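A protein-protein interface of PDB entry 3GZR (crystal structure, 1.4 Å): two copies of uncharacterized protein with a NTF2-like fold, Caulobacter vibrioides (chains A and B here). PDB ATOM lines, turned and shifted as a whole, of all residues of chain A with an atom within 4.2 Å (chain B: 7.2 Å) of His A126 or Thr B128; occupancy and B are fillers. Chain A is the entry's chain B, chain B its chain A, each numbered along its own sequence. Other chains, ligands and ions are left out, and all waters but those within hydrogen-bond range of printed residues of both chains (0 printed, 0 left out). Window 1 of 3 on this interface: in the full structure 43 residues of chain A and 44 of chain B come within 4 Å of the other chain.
Printed residues of chain B within 4 Å of Val A38: Val B86 (3.998 Å) and Arg B108 (3.8 Å). Of the printed residues of chain B, Asn A39 touches Thr B128 (3.6 Å). Of the printed residues of chain B, Thr A110 touches His B124 (2.7 Å) and His B126 (2.6 Å). Printed residues of chain B within 4 Å of His A124: Val B86 and Thr B110. His A126 touches just these residues of chain B: Arg B108, Thr B110, His B126, Asn B127 and Thr B128. Of the printed residues of chain A, Asn B39 touches Thr A128 (3.5 Å). Val B87 touches none of the printed residues of chain A. Gly B125 touches none of the printed residues of chain A. Of chain A, only Asn A39 (3.6 Å), Val A40 (3.3 Å), Gly A42 (3.8 Å), His A126 (2.7 Å), Asn A127 (3.0 Å) and Thr A128 (2.8 Å) come within 4 Å of Thr B128.
Hydrophobic or aromatic side chains of chain B that line the printed part of chain A: Val B38, Val B86, His B124 and His B126. Of the 12 printed residues of chain A, 10 touch a printed residue of chain B. Among the printed residues, no Asp or Glu carboxylate lies within 4 Å of a Lys or Arg side-chain nitrogen of the other chain.
O of His B126 sits close to ND1 of His A126 (3.4 Å). The side-chain hydroxyl (OG1) of Thr B128 is in hydrogen-bond range of a ring nitrogen (NE2) of His A126, 2.7 Å away. A ring nitrogen (ND1) of His A126 lies within hydrogen-bond range of the side-chain hydroxyl (OG1) of Thr B110, at 2.6 Å. The side-chain hydroxyl (OG1) of Thr B110 sits at hydrogen-bond distance from a ring nitrogen (NE2) of His A124 (2.7 Å). The backbone carbonyl oxygen of Arg A108 lies close to a ring nitrogen (NE2) of His B126. The backbone carbonyl oxygen (O) of Arg B108 sits close to a ring nitrogen (NE2) of His A126 (3.4 Å). The side-chain hydroxyl (OG1) of Thr A128 is in hydrogen-bond range of a ring nitrogen (NE2) of His B126, at 2.8 Å. OG1 of Thr B128 is in hydrogen-bond range of O of Asn A127 (3.0 Å). NE2 of His B124 lies within hydrogen-bond range of OG1 of Thr A110. The backbone carbonyl oxygen (O) of Asn B127 lies within hydrogen-bond range of the side-chain hydroxyl (OG1) of Thr A128 (2.9 Å). O of Gly A42 sits at hydrogen-bond distance from NE of Arg B108, at 2.8 Å. OG1 of Thr B128 sits at hydrogen-bond distance from OG1 of Thr A128. ND1 of His B126 sits at hydrogen-bond distance from OG1 of Thr A110 (2.6 Å).
Val A38 touches Val B86. CG1 of Val A38 touches CG of Arg B108 (3.8 Å). Thr B128 touches Asn A39. Val A40 touches Thr B128 (O to CG2, 3.3 Å). Thr B128 touches Gly A42 (CG2 to N, 3.8 Å). CG1 of Val B38 touches CG of Arg A108, 3.8 Å away. Val B86 touches His A124. His A126 touches Asn B127. Asn A127 touches His B126. Asn B39 touches Thr A128.
Asn A39 touches Thr B128, and with the chains exchanged Thr A128 touches Asn B39. His A126 touches Thr B128, and with the chains exchanged Thr A128 touches His B126. Asn A127 touches Thr B128, and with the chains exchanged Thr A128 touches Asn B127. Thr B128 touches its own counterpart, Thr A128. Of the 24 pairs that touch across the chains among the printed residues, 20 have their exchanged pair printed and touching as well.
O of Thr A128 sits at hydrogen-bond distance from N of Arg A108. O of Arg A108 sits close to OD1 of Asn A127 (3.2 Å). The backbone NH (N) of Val A38 lies within hydrogen-bond range of the backbone carbonyl oxygen (O) of Gly A125. N of Val B38 sits at hydrogen-bond distance from O of Gly B125, 2.9 Å away. The side-chain amide oxygen (OD1) of Asn A39 sits at hydrogen-bond distance from the backbone NH (N) of Gly A42, at 3.2 Å. The backbone NH (N) of Arg B108 sits at hydrogen-bond distance from the backbone carbonyl oxygen (O) of Thr B128, 2.8 Å away.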
ATOM      1  N   VAL A  38      -8.997  12.167 -18.374  1.00  0.00           N
ATOM      2  CA  VAL A  38      -7.534  12.113 -18.165  1.00  0.00           C
ATOM      3  C   VAL A  38      -7.106  13.513 -17.688  1.00  0.00           C
ATOM      4  O   VAL A  38      -7.388  14.500 -18.339  1.00  0.00           O
ATOM      5  CB  VAL A  38      -6.752  11.683 -19.400  1.00  0.00           C
ATOM      6  CG1 VAL A  38      -5.228  11.681 -19.067  1.00  0.00           C
ATOM      7  CG2 VAL A  38      -7.199  10.323 -19.894  1.00  0.00           C
ATOM      8  N   ASN A  39      -6.497  13.564 -16.488  1.00  0.00           N
ATOM      9  CA  ASN A  39      -6.096  14.841 -15.902  1.00  0.00           C
ATOM     10  C   ASN A  39      -4.660  15.234 -16.277  1.00  0.00           C
ATOM     11  O   ASN A  39      -3.957  14.525 -17.003  1.00  0.00           O
ATOM     12  CB  ASN A  39      -6.392  14.879 -14.387  1.00  0.00           C
ATOM     13  CG  ASN A  39      -5.282  14.300 -13.540  1.00  0.00           C
ATOM     14  OD1 ASN A  39      -4.383  13.605 -14.032  1.00  0.00           O
ATOM     15  ND2 ASN A  39      -5.331  14.621 -12.220  1.00  0.00           N
ATOM     16  N   VAL A  40      -4.222  16.376 -15.727  1.00  0.00           N
ATOM     17  CA  VAL A  40      -2.945  17.021 -16.092  1.00  0.00           C
ATOM     18  C   VAL A  40      -1.704  16.195 -15.752  1.00  0.00           C
ATOM     19  O   VAL A  40      -0.629  16.495 -16.280  1.00  0.00           O
ATOM     20  CB  VAL A  40      -2.756  18.445 -15.540  1.00  0.00           C
ATOM     21  CG1 VAL A  40      -3.804  19.399 -16.175  1.00  0.00           C
ATOM     22  CG2 VAL A  40      -2.798  18.418 -14.003  1.00  0.00           C
ATOM     23  N   GLY A  42      -1.946  12.738 -15.934  1.00  0.00           N
ATOM     24  CA  GLY A  42      -2.171  11.456 -16.573  1.00  0.00           C
ATOM     25  C   GLY A  42      -3.020  10.473 -15.804  1.00  0.00           C
ATOM     26  O   GLY A  42      -3.097   9.316 -16.183  1.00  0.00           O
ATOM     27  N   ARG A 108      -4.704  23.366 -21.607  1.00  0.00           N
ATOM     28  CA  ARG A 108      -5.350  23.055 -22.884  1.00  0.00           C
ATOM     29  C   ARG A 108      -6.190  21.813 -22.623  1.00  0.00           C
ATOM     30  O   ARG A 108      -5.660  20.728 -22.411  1.00  0.00           O
ATOM     31  CB  ARG A 108      -4.332  22.846 -24.006  1.00  0.00           C
ATOM     32  CG  ARG A 108      -4.920  23.076 -25.407  1.00  0.00           C
ATOM     33  CD  ARG A 108      -4.900  24.555 -25.756  1.00  0.00           C
ATOM     34  NE  ARG A 108      -3.511  24.974 -25.990  1.00  0.00           N
ATOM     35  CZ  ARG A 108      -3.047  26.222 -25.997  1.00  0.00           C
ATOM     36  NH1 ARG A 108      -3.853  27.265 -25.774  1.00  0.00           N
ATOM     37  NH2 ARG A 108      -1.743  26.432 -26.209  1.00  0.00           N
ATOM     38  N   LEU A 109      -7.509  21.984 -22.643  1.00  0.00           N
ATOM     39  CA  LEU A 109      -8.451  20.975 -22.233  1.00  0.00           C
ATOM     40  C   LEU A 109      -9.341  20.547 -23.406  1.00  0.00           C
ATOM     41  O   LEU A 109     -10.058  21.387 -23.997  1.00  0.00           O
ATOM     42  CB  LEU A 109      -9.313  21.538 -21.102  1.00  0.00           C
ATOM     43  CG  LEU A 109     -10.499  20.718 -20.600  1.00  0.00           C
ATOM     44  CD1 LEU A 109     -10.041  19.429 -19.913  1.00  0.00           C
ATOM     45  CD2 LEU A 109     -11.432  21.532 -19.663  1.00  0.00           C
ATOM     46  N   THR A 110      -9.330  19.250 -23.683  1.00  0.00           N
ATOM     47  CA  THR A 110     -10.271  18.633 -24.627  1.00  0.00           C
ATOM     48  C   THR A 110     -11.525  18.286 -23.880  1.00  0.00           C
ATOM     49  O   THR A 110     -11.467  17.637 -22.829  1.00  0.00           O
ATOM     50  CB  THR A 110      -9.684  17.353 -25.281  1.00  0.00           C
ATOM     51  OG1 THR A 110      -8.695  17.762 -26.216  1.00  0.00           O
ATOM     52  CG2 THR A 110     -10.757  16.486 -25.990  1.00  0.00           C
ATOM     53  N   HIS A 124     -16.162  12.668 -22.364  1.00  0.00           N
ATOM     54  CA  HIS A 124     -14.735  12.612 -22.092  1.00  0.00           C
ATOM     55  C   HIS A 124     -14.128  13.981 -21.945  1.00  0.00           C
ATOM     56  O   HIS A 124     -14.559  14.958 -22.571  1.00  0.00           O
ATOM     57  CB  HIS A 124     -14.056  11.887 -23.261  1.00  0.00           C
ATOM     58  CG  HIS A 124     -12.623  11.536 -23.056  1.00  0.00           C
ATOM     59  ND1 HIS A 124     -12.202  10.619 -22.114  1.00  0.00           N
ATOM     60  CD2 HIS A 124     -11.507  11.996 -23.678  1.00  0.00           C
ATOM     61  CE1 HIS A 124     -10.886  10.507 -22.203  1.00  0.00           C
ATOM     62  NE2 HIS A 124     -10.429  11.336 -23.126  1.00  0.00           N
ATOM     63  N   GLY A 125     -13.081  14.056 -21.126  1.00  0.00           N
ATOM     64  CA  GLY A 125     -12.234  15.232 -21.010  1.00  0.00           C
ATOM     65  C   GLY A 125     -10.794  14.808 -20.846  1.00  0.00           C
ATOM     66  O   GLY A 125     -10.519  13.707 -20.359  1.00  0.00           O
ATOM     67  N   HIS A 126      -9.886  15.631 -21.340  1.00  0.00           N
ATOM     68  CA  HIS A 126      -8.454  15.353 -21.245  1.00  0.00           C
ATOM     69  C   HIS A 126      -7.747  16.708 -21.113  1.00  0.00           C
ATOM     70  O   HIS A 126      -7.904  17.561 -21.966  1.00  0.00           O
ATOM     71  CB  HIS A 126      -8.022  14.569 -22.466  1.00  0.00           C
ATOM     72  CG  HIS A 126      -6.632  13.984 -22.369  1.00  0.00           C
ATOM     73  ND1 HIS A 126      -6.318  12.733 -22.843  1.00  0.00           N
ATOM     74  CD2 HIS A 126      -5.486  14.494 -21.847  1.00  0.00           C
ATOM     75  CE1 HIS A 126      -5.029  12.506 -22.634  1.00  0.00           C
ATOM     76  NE2 HIS A 126      -4.498  13.553 -22.043  1.00  0.00           N
ATOM     77  N   ASN A 127      -6.932  16.869 -20.069  1.00  0.00           N
ATOM     78  CA  ASN A 127      -6.288  18.128 -19.799  1.00  0.00           C
ATOM     79  C   ASN A 127      -4.772  17.987 -19.841  1.00  0.00           C
ATOM     80  O   ASN A 127      -4.210  16.965 -19.421  1.00  0.00           O
ATOM     81  CB  ASN A 127      -6.725  18.652 -18.413  1.00  0.00           C
ATOM     82  CG  ASN A 127      -6.608  20.153 -18.276  1.00  0.00           C
ATOM     83  OD1 ASN A 127      -6.229  20.847 -19.235  1.00  0.00           O
ATOM     84  ND2 ASN A 127      -6.940  20.670 -17.091  1.00  0.00           N
ATOM     85  N   THR A 128      -4.121  19.032 -20.351  1.00  0.00           N
ATOM     86  CA  THR A 128      -2.640  19.157 -20.402  1.00  0.00           C
ATOM     87  C   THR A 128      -2.243  20.583 -20.042  1.00  0.00           C
ATOM     88  O   THR A 128      -2.894  21.530 -20.473  1.00  0.00           O
ATOM     89  CB  THR A 128      -2.088  18.822 -21.792  1.00  0.00           C
ATOM     90  OG1 THR A 128      -2.472  17.487 -22.120  1.00  0.00           O
ATOM     91  CG2 THR A 128      -0.553  18.897 -21.854  1.00  0.00           C
ATOM     92  N   VAL B  38      -3.682  17.896 -29.578  1.00  0.00           N
ATOM     93  CA  VAL B  38      -3.058  18.629 -28.467  1.00  0.00           C
ATOM     94  C   VAL B  38      -1.922  17.773 -27.927  1.00  0.00           C
ATOM     95  O   VAL B  38      -2.158  16.621 -27.566  1.00  0.00           O
ATOM     96  CB  VAL B  38      -4.018  18.962 -27.334  1.00  0.00           C
ATOM     97  CG1 VAL B  38      -3.272  19.701 -26.185  1.00  0.00           C
ATOM     98  CG2 VAL B  38      -5.211  19.844 -27.824  1.00  0.00           C
ATOM     99  N   ASN B  39      -0.686  18.286 -27.943  1.00  0.00           N
ATOM    100  CA  ASN B  39       0.467  17.484 -27.521  1.00  0.00           C
ATOM    101  C   ASN B  39       0.789  17.638 -26.025  1.00  0.00           C
ATOM    102  O   ASN B  39       0.102  18.350 -25.289  1.00  0.00           O
ATOM    103  CB  ASN B  39       1.661  17.747 -28.450  1.00  0.00           C
ATOM    104  CG  ASN B  39       2.477  18.946 -28.065  1.00  0.00           C
ATOM    105  OD1 ASN B  39       2.077  19.791 -27.250  1.00  0.00           O
ATOM    106  ND2 ASN B  39       3.676  19.048 -28.662  1.00  0.00           N
ATOM    107  N   VAL B  40       1.868  16.969 -25.596  1.00  0.00           N
ATOM    108  CA  VAL B  40       2.224  16.887 -24.176  1.00  0.00           C
ATOM    109  C   VAL B  40       2.580  18.215 -23.510  1.00  0.00           C
ATOM    110  O   VAL B  40       2.608  18.296 -22.275  1.00  0.00           O
ATOM    111  CB  VAL B  40       3.371  15.886 -23.921  1.00  0.00           C
ATOM    112  CG1 VAL B  40       2.949  14.464 -24.247  1.00  0.00           C
ATOM    113  CG2 VAL B  40       4.696  16.294 -24.643  1.00  0.00           C
ATOM    114  N   VAL B  41       2.911  19.243 -24.304  1.00  0.00           N
ATOM    115  CA  VAL B  41       3.223  20.585 -23.806  1.00  0.00           C
ATOM    116  C   VAL B  41       2.087  21.585 -24.127  1.00  0.00           C
ATOM    117  O   VAL B  41       2.255  22.775 -23.961  1.00  0.00           O
ATOM    118  CB  VAL B  41       4.618  21.090 -24.263  1.00  0.00           C
ATOM    119  CG1 VAL B  41       5.708  20.362 -23.455  1.00  0.00           C
ATOM    120  CG2 VAL B  41       4.846  20.908 -25.752  1.00  0.00           C
ATOM    121  N   ALA B  85     -10.488   5.951 -27.539  1.00  0.00           N
ATOM    122  CA  ALA B  85      -9.493   5.163 -26.846  1.00  0.00           C
ATOM    123  C   ALA B  85      -8.665   5.997 -25.901  1.00  0.00           C
ATOM    124  O   ALA B  85      -8.287   7.128 -26.235  1.00  0.00           O
ATOM    125  CB  ALA B  85      -8.546   4.473 -27.864  1.00  0.00           C
ATOM    126  N   VAL B  86      -8.357   5.421 -24.734  1.00  0.00           N
ATOM    127  CA  VAL B  86      -7.354   5.974 -23.816  1.00  0.00           C
ATOM    128  C   VAL B  86      -6.210   4.972 -23.861  1.00  0.00           C
ATOM    129  O   VAL B  86      -6.364   3.810 -23.488  1.00  0.00           O
ATOM    130  CB  VAL B  86      -7.870   6.197 -22.423  1.00  0.00           C
ATOM    131  CG1 VAL B  86      -6.730   6.714 -21.548  1.00  0.00           C
ATOM    132  CG2 VAL B  86      -9.039   7.246 -22.454  1.00  0.00           C
ATOM    133  N   VAL B  87      -5.090   5.446 -24.370  1.00  0.00           N
ATOM    134  CA  VAL B  87      -3.890   4.646 -24.646  1.00  0.00           C
ATOM    135  C   VAL B  87      -2.848   4.956 -23.608  1.00  0.00           C
ATOM    136  O   VAL B  87      -2.581   6.128 -23.301  1.00  0.00           O
ATOM    137  CB  VAL B  87      -3.376   4.968 -26.051  1.00  0.00           C
ATOM    138  CG1 VAL B  87      -2.074   4.147 -26.384  1.00  0.00           C
ATOM    139  CG2 VAL B  87      -4.494   4.707 -27.096  1.00  0.00           C
ATOM    140  N   LEU B  89       1.182   4.436 -23.085  1.00  0.00           N
ATOM    141  CA  LEU B  89       2.389   4.111 -23.815  1.00  0.00           C
ATOM    142  C   LEU B  89       3.589   4.460 -22.981  1.00  0.00           C
ATOM    143  O   LEU B  89       3.497   5.223 -22.028  1.00  0.00           O
ATOM    144  CB  LEU B  89       2.423   4.803 -25.163  1.00  0.00           C
ATOM    145  CG  LEU B  89       2.355   6.295 -25.132  1.00  0.00           C
ATOM    146  CD1 LEU B  89       3.346   6.946 -26.090  1.00  0.00           C
ATOM    147  CD2 LEU B  89       0.914   6.830 -25.466  1.00  0.00           C
ATOM    148  N   HIS B 106       5.767   7.095 -18.979  1.00  0.00           N
ATOM    149  CA  HIS B 106       4.489   6.724 -19.534  1.00  0.00           C
ATOM    150  C   HIS B 106       3.751   8.004 -19.962  1.00  0.00           C
ATOM    151  O   HIS B 106       3.849   9.040 -19.283  1.00  0.00           O
ATOM    152  CB  HIS B 106       3.638   5.988 -18.539  1.00  0.00           C
ATOM    153  CG  HIS B 106       4.096   4.594 -18.240  1.00  0.00           C
ATOM    154  ND1 HIS B 106       5.325   4.300 -17.677  1.00  0.00           N
ATOM    155  CD2 HIS B 106       3.455   3.414 -18.390  1.00  0.00           C
ATOM    156  CE1 HIS B 106       5.408   2.989 -17.486  1.00  0.00           C
ATOM    157  NE2 HIS B 106       4.294   2.427 -17.913  1.00  0.00           N
ATOM    158  N   ASP B 107       3.052   7.906 -21.088  1.00  0.00           N
ATOM    159  CA  ASP B 107       2.128   8.935 -21.553  1.00  0.00           C
ATOM    160  C   ASP B 107       0.716   8.341 -21.546  1.00  0.00           C
ATOM    161  O   ASP B 107       0.543   7.142 -21.742  1.00  0.00           O
ATOM    162  CB  ASP B 107       2.422   9.397 -22.969  1.00  0.00           C
ATOM    163  CG  ASP B 107       3.781  10.002 -23.187  1.00  0.00           C
ATOM    164  OD1 ASP B 107       4.474  10.393 -22.255  1.00  0.00           O
ATOM    165  OD2 ASP B 107       4.137  10.055 -24.427  1.00  0.00           O
ATOM    166  N   ARG B 108      -0.271   9.222 -21.382  1.00  0.00           N
ATOM    167  CA  ARG B 108      -1.687   8.877 -21.421  1.00  0.00           C
ATOM    168  C   ARG B 108      -2.275   9.662 -22.588  1.00  0.00           C
ATOM    169  O   ARG B 108      -2.389  10.901 -22.501  1.00  0.00           O
ATOM    170  CB  ARG B 108      -2.402   9.178 -20.090  1.00  0.00           C
ATOM    171  CG  ARG B 108      -3.638   8.309 -19.916  1.00  0.00           C
ATOM    172  CD  ARG B 108      -3.295   6.956 -19.324  1.00  0.00           C
ATOM    173  NE  ARG B 108      -2.897   7.140 -17.929  1.00  0.00           N
ATOM    174  CZ  ARG B 108      -2.239   6.246 -17.188  1.00  0.00           C
ATOM    175  NH1 ARG B 108      -1.903   5.044 -17.686  1.00  0.00           N
ATOM    176  NH2 ARG B 108      -1.882   6.563 -15.933  1.00  0.00           N
ATOM    177  N   LEU B 109      -2.665   8.955 -23.650  1.00  0.00           N
ATOM    178  CA  LEU B 109      -3.071   9.530 -24.920  1.00  0.00           C
ATOM    179  C   LEU B 109      -4.532   9.201 -25.248  1.00  0.00           C
ATOM    180  O   LEU B 109      -4.916   8.049 -25.317  1.00  0.00           O
ATOM    181  CB  LEU B 109      -2.130   8.990 -26.002  1.00  0.00           C
ATOM    182  CG  LEU B 109      -2.432   9.274 -27.482  1.00  0.00           C
ATOM    183  CD1 LEU B 109      -2.327  10.768 -27.820  1.00  0.00           C
ATOM    184  CD2 LEU B 109      -1.523   8.435 -28.381  1.00  0.00           C
ATOM    185  N   THR B 110      -5.332  10.250 -25.410  1.00  0.00           N
ATOM    186  CA  THR B 110      -6.691  10.089 -25.935  1.00  0.00           C
ATOM    187  C   THR B 110      -6.648  10.118 -27.446  1.00  0.00           C
ATOM    188  O   THR B 110      -6.015  10.971 -28.046  1.00  0.00           O
ATOM    189  CB  THR B 110      -7.620  11.236 -25.471  1.00  0.00           C
ATOM    190  OG1 THR B 110      -7.883  11.080 -24.080  1.00  0.00           O
ATOM    191  CG2 THR B 110      -8.943  11.304 -26.260  1.00  0.00           C
ATOM    192  N   LEU B 111      -7.337   9.162 -28.059  1.00  0.00           N
ATOM    193  CA  LEU B 111      -7.546   9.161 -29.526  1.00  0.00           C
ATOM    194  C   LEU B 111      -9.029   8.960 -29.792  1.00  0.00           C
ATOM    195  O   LEU B 111      -9.683   8.111 -29.154  1.00  0.00           O
ATOM    196  CB  LEU B 111      -6.693   8.115 -30.219  1.00  0.00           C
ATOM    197  CG  LEU B 111      -5.220   8.471 -30.330  1.00  0.00           C
ATOM    198  CD1 LEU B 111      -4.341   7.240 -30.639  1.00  0.00           C
ATOM    199  CD2 LEU B 111      -4.974   9.544 -31.399  1.00  0.00           C
ATOM    200  N   HIS B 124      -9.197  13.307 -33.610  1.00  0.00           N
ATOM    201  CA  HIS B 124      -8.538  14.054 -32.553  1.00  0.00           C
ATOM    202  C   HIS B 124      -7.629  13.179 -31.733  1.00  0.00           C
ATOM    203  O   HIS B 124      -7.896  12.010 -31.527  1.00  0.00           O
ATOM    204  CB  HIS B 124      -9.615  14.675 -31.641  1.00  0.00           C
ATOM    205  CG  HIS B 124      -9.107  15.601 -30.582  1.00  0.00           C
ATOM    206  ND1 HIS B 124      -8.559  16.831 -30.881  1.00  0.00           N
ATOM    207  CD2 HIS B 124      -9.142  15.514 -29.226  1.00  0.00           C
ATOM    208  CE1 HIS B 124      -8.277  17.462 -29.749  1.00  0.00           C
ATOM    209  NE2 HIS B 124      -8.583  16.666 -28.726  1.00  0.00           N
ATOM    210  N   GLY B 125      -6.529  13.780 -31.270  1.00  0.00           N
ATOM    211  CA  GLY B 125      -5.648  13.178 -30.272  1.00  0.00           C
ATOM    212  C   GLY B 125      -5.289  14.211 -29.213  1.00  0.00           C
ATOM    213  O   GLY B 125      -5.252  15.401 -29.494  1.00  0.00           O
ATOM    214  N   HIS B 126      -5.008  13.745 -27.994  1.00  0.00           N
ATOM    215  CA  HIS B 126      -4.615  14.617 -26.901  1.00  0.00           C
ATOM    216  C   HIS B 126      -3.712  13.798 -25.975  1.00  0.00           C
ATOM    217  O   HIS B 126      -4.124  12.766 -25.502  1.00  0.00           O
ATOM    218  CB  HIS B 126      -5.843  15.135 -26.148  1.00  0.00           C
ATOM    219  CG  HIS B 126      -5.552  16.252 -25.196  1.00  0.00           C
ATOM    220  ND1 HIS B 126      -6.362  17.359 -25.071  1.00  0.00           N
ATOM    221  CD2 HIS B 126      -4.544  16.418 -24.316  1.00  0.00           C
ATOM    222  CE1 HIS B 126      -5.864  18.145 -24.135  1.00  0.00           C
ATOM    223  NE2 HIS B 126      -4.759  17.606 -23.662  1.00  0.00           N
ATOM    224  N   ASN B 127      -2.489  14.277 -25.741  1.00  0.00           N
ATOM    225  CA  ASN B 127      -1.486  13.545 -24.972  1.00  0.00           C
ATOM    226  C   ASN B 127      -1.086  14.307 -23.713  1.00  0.00           C
ATOM    227  O   ASN B 127      -1.003  15.540 -23.716  1.00  0.00           O
ATOM    228  CB  ASN B 127      -0.276  13.252 -25.866  1.00  0.00           C
ATOM    229  CG  ASN B 127       0.522  12.055 -25.439  1.00  0.00           C
ATOM    230  OD1 ASN B 127       0.181  11.331 -24.517  1.00  0.00           O
ATOM    231  ND2 ASN B 127       1.632  11.825 -26.171  1.00  0.00           N
ATOM    232  N   THR B 128      -0.807  13.545 -22.664  1.00  0.00           N
ATOM    233  CA  THR B 128      -0.322  14.056 -21.370  1.00  0.00           C
ATOM    234  C   THR B 128       0.732  13.101 -20.824  1.00  0.00           C
ATOM    235  O   THR B 128       0.567  11.905 -20.946  1.00  0.00           O
ATOM    236  CB  THR B 128      -1.464  14.139 -20.332  1.00  0.00           C
ATOM    237  OG1 THR B 128      -2.501  14.983 -20.871  1.00  0.00           O
ATOM    238  CG2 THR B 128      -0.984  14.746 -19.021  1.00  0.00           C
ATOM    239  N   ILE B 129       1.800  13.622 -20.234  1.00  0.00           N
ATOM    240  CA  ILE B 129       2.823  12.774 -19.604  1.00  0.00           C
ATOM    241  C   ILE B 129       2.272  12.325 -18.236  1.00  0.00           C
ATOM    242  O   ILE B 129       1.740  13.154 -17.465  1.00  0.00           O
ATOM    243  CB  ILE B 129       4.145  13.542 -19.441  1.00  0.00           C
ATOM    244  CG1 ILE B 129       4.660  13.976 -20.805  1.00  0.00           C
ATOM    245  CG2 ILE B 129       5.179  12.662 -18.676  1.00  0.00           C
ATOM    246  CD1 ILE B 129       5.871  14.905 -20.788  1.00  0.00           C
ATOM    247  N   VAL B 130       2.422  11.044 -17.911  1.00  0.00           N
ATOM    248  CA  VAL B 130       2.009  10.541 -16.589  1.00  0.00           C
ATOM    249  C   VAL B 130       3.104  10.905 -15.586  1.00  0.00           C
ATOM    250  O   VAL B 130       4.261  10.532 -15.759  1.00  0.00           O
ATOM    251  CB  VAL B 130       1.802   9.024 -16.625  1.00  0.00           C
ATOM    252  CG1 VAL B 130       1.481   8.448 -15.242  1.00  0.00           C
ATOM    253  CG2 VAL B 130       0.703   8.631 -17.643  1.00  0.00           C
ATOM    254  N   ASN B 131       2.735  11.624 -14.532  1.00  0.00           N
ATOM    255  CA  ASN B 131       3.681  11.985 -13.475  1.00  0.00           C
ATOM    256  C   ASN B 131       3.722  10.820 -12.480  1.00  0.00           C
ATOM    257  O   ASN B 131       2.764  10.583 -11.773  1.00  0.00           O
ATOM    258  CB  ASN B 131       3.256  13.277 -12.787  1.00  0.00           C
ATOM    259  CG  ASN B 131       4.286  13.763 -11.816  1.00  0.00           C
ATOM    260  OD1 ASN B 131       4.971  12.952 -11.194  1.00  0.00           O
ATOM    261  ND2 ASN B 131       4.413  15.083 -11.645  1.00  0.00           N
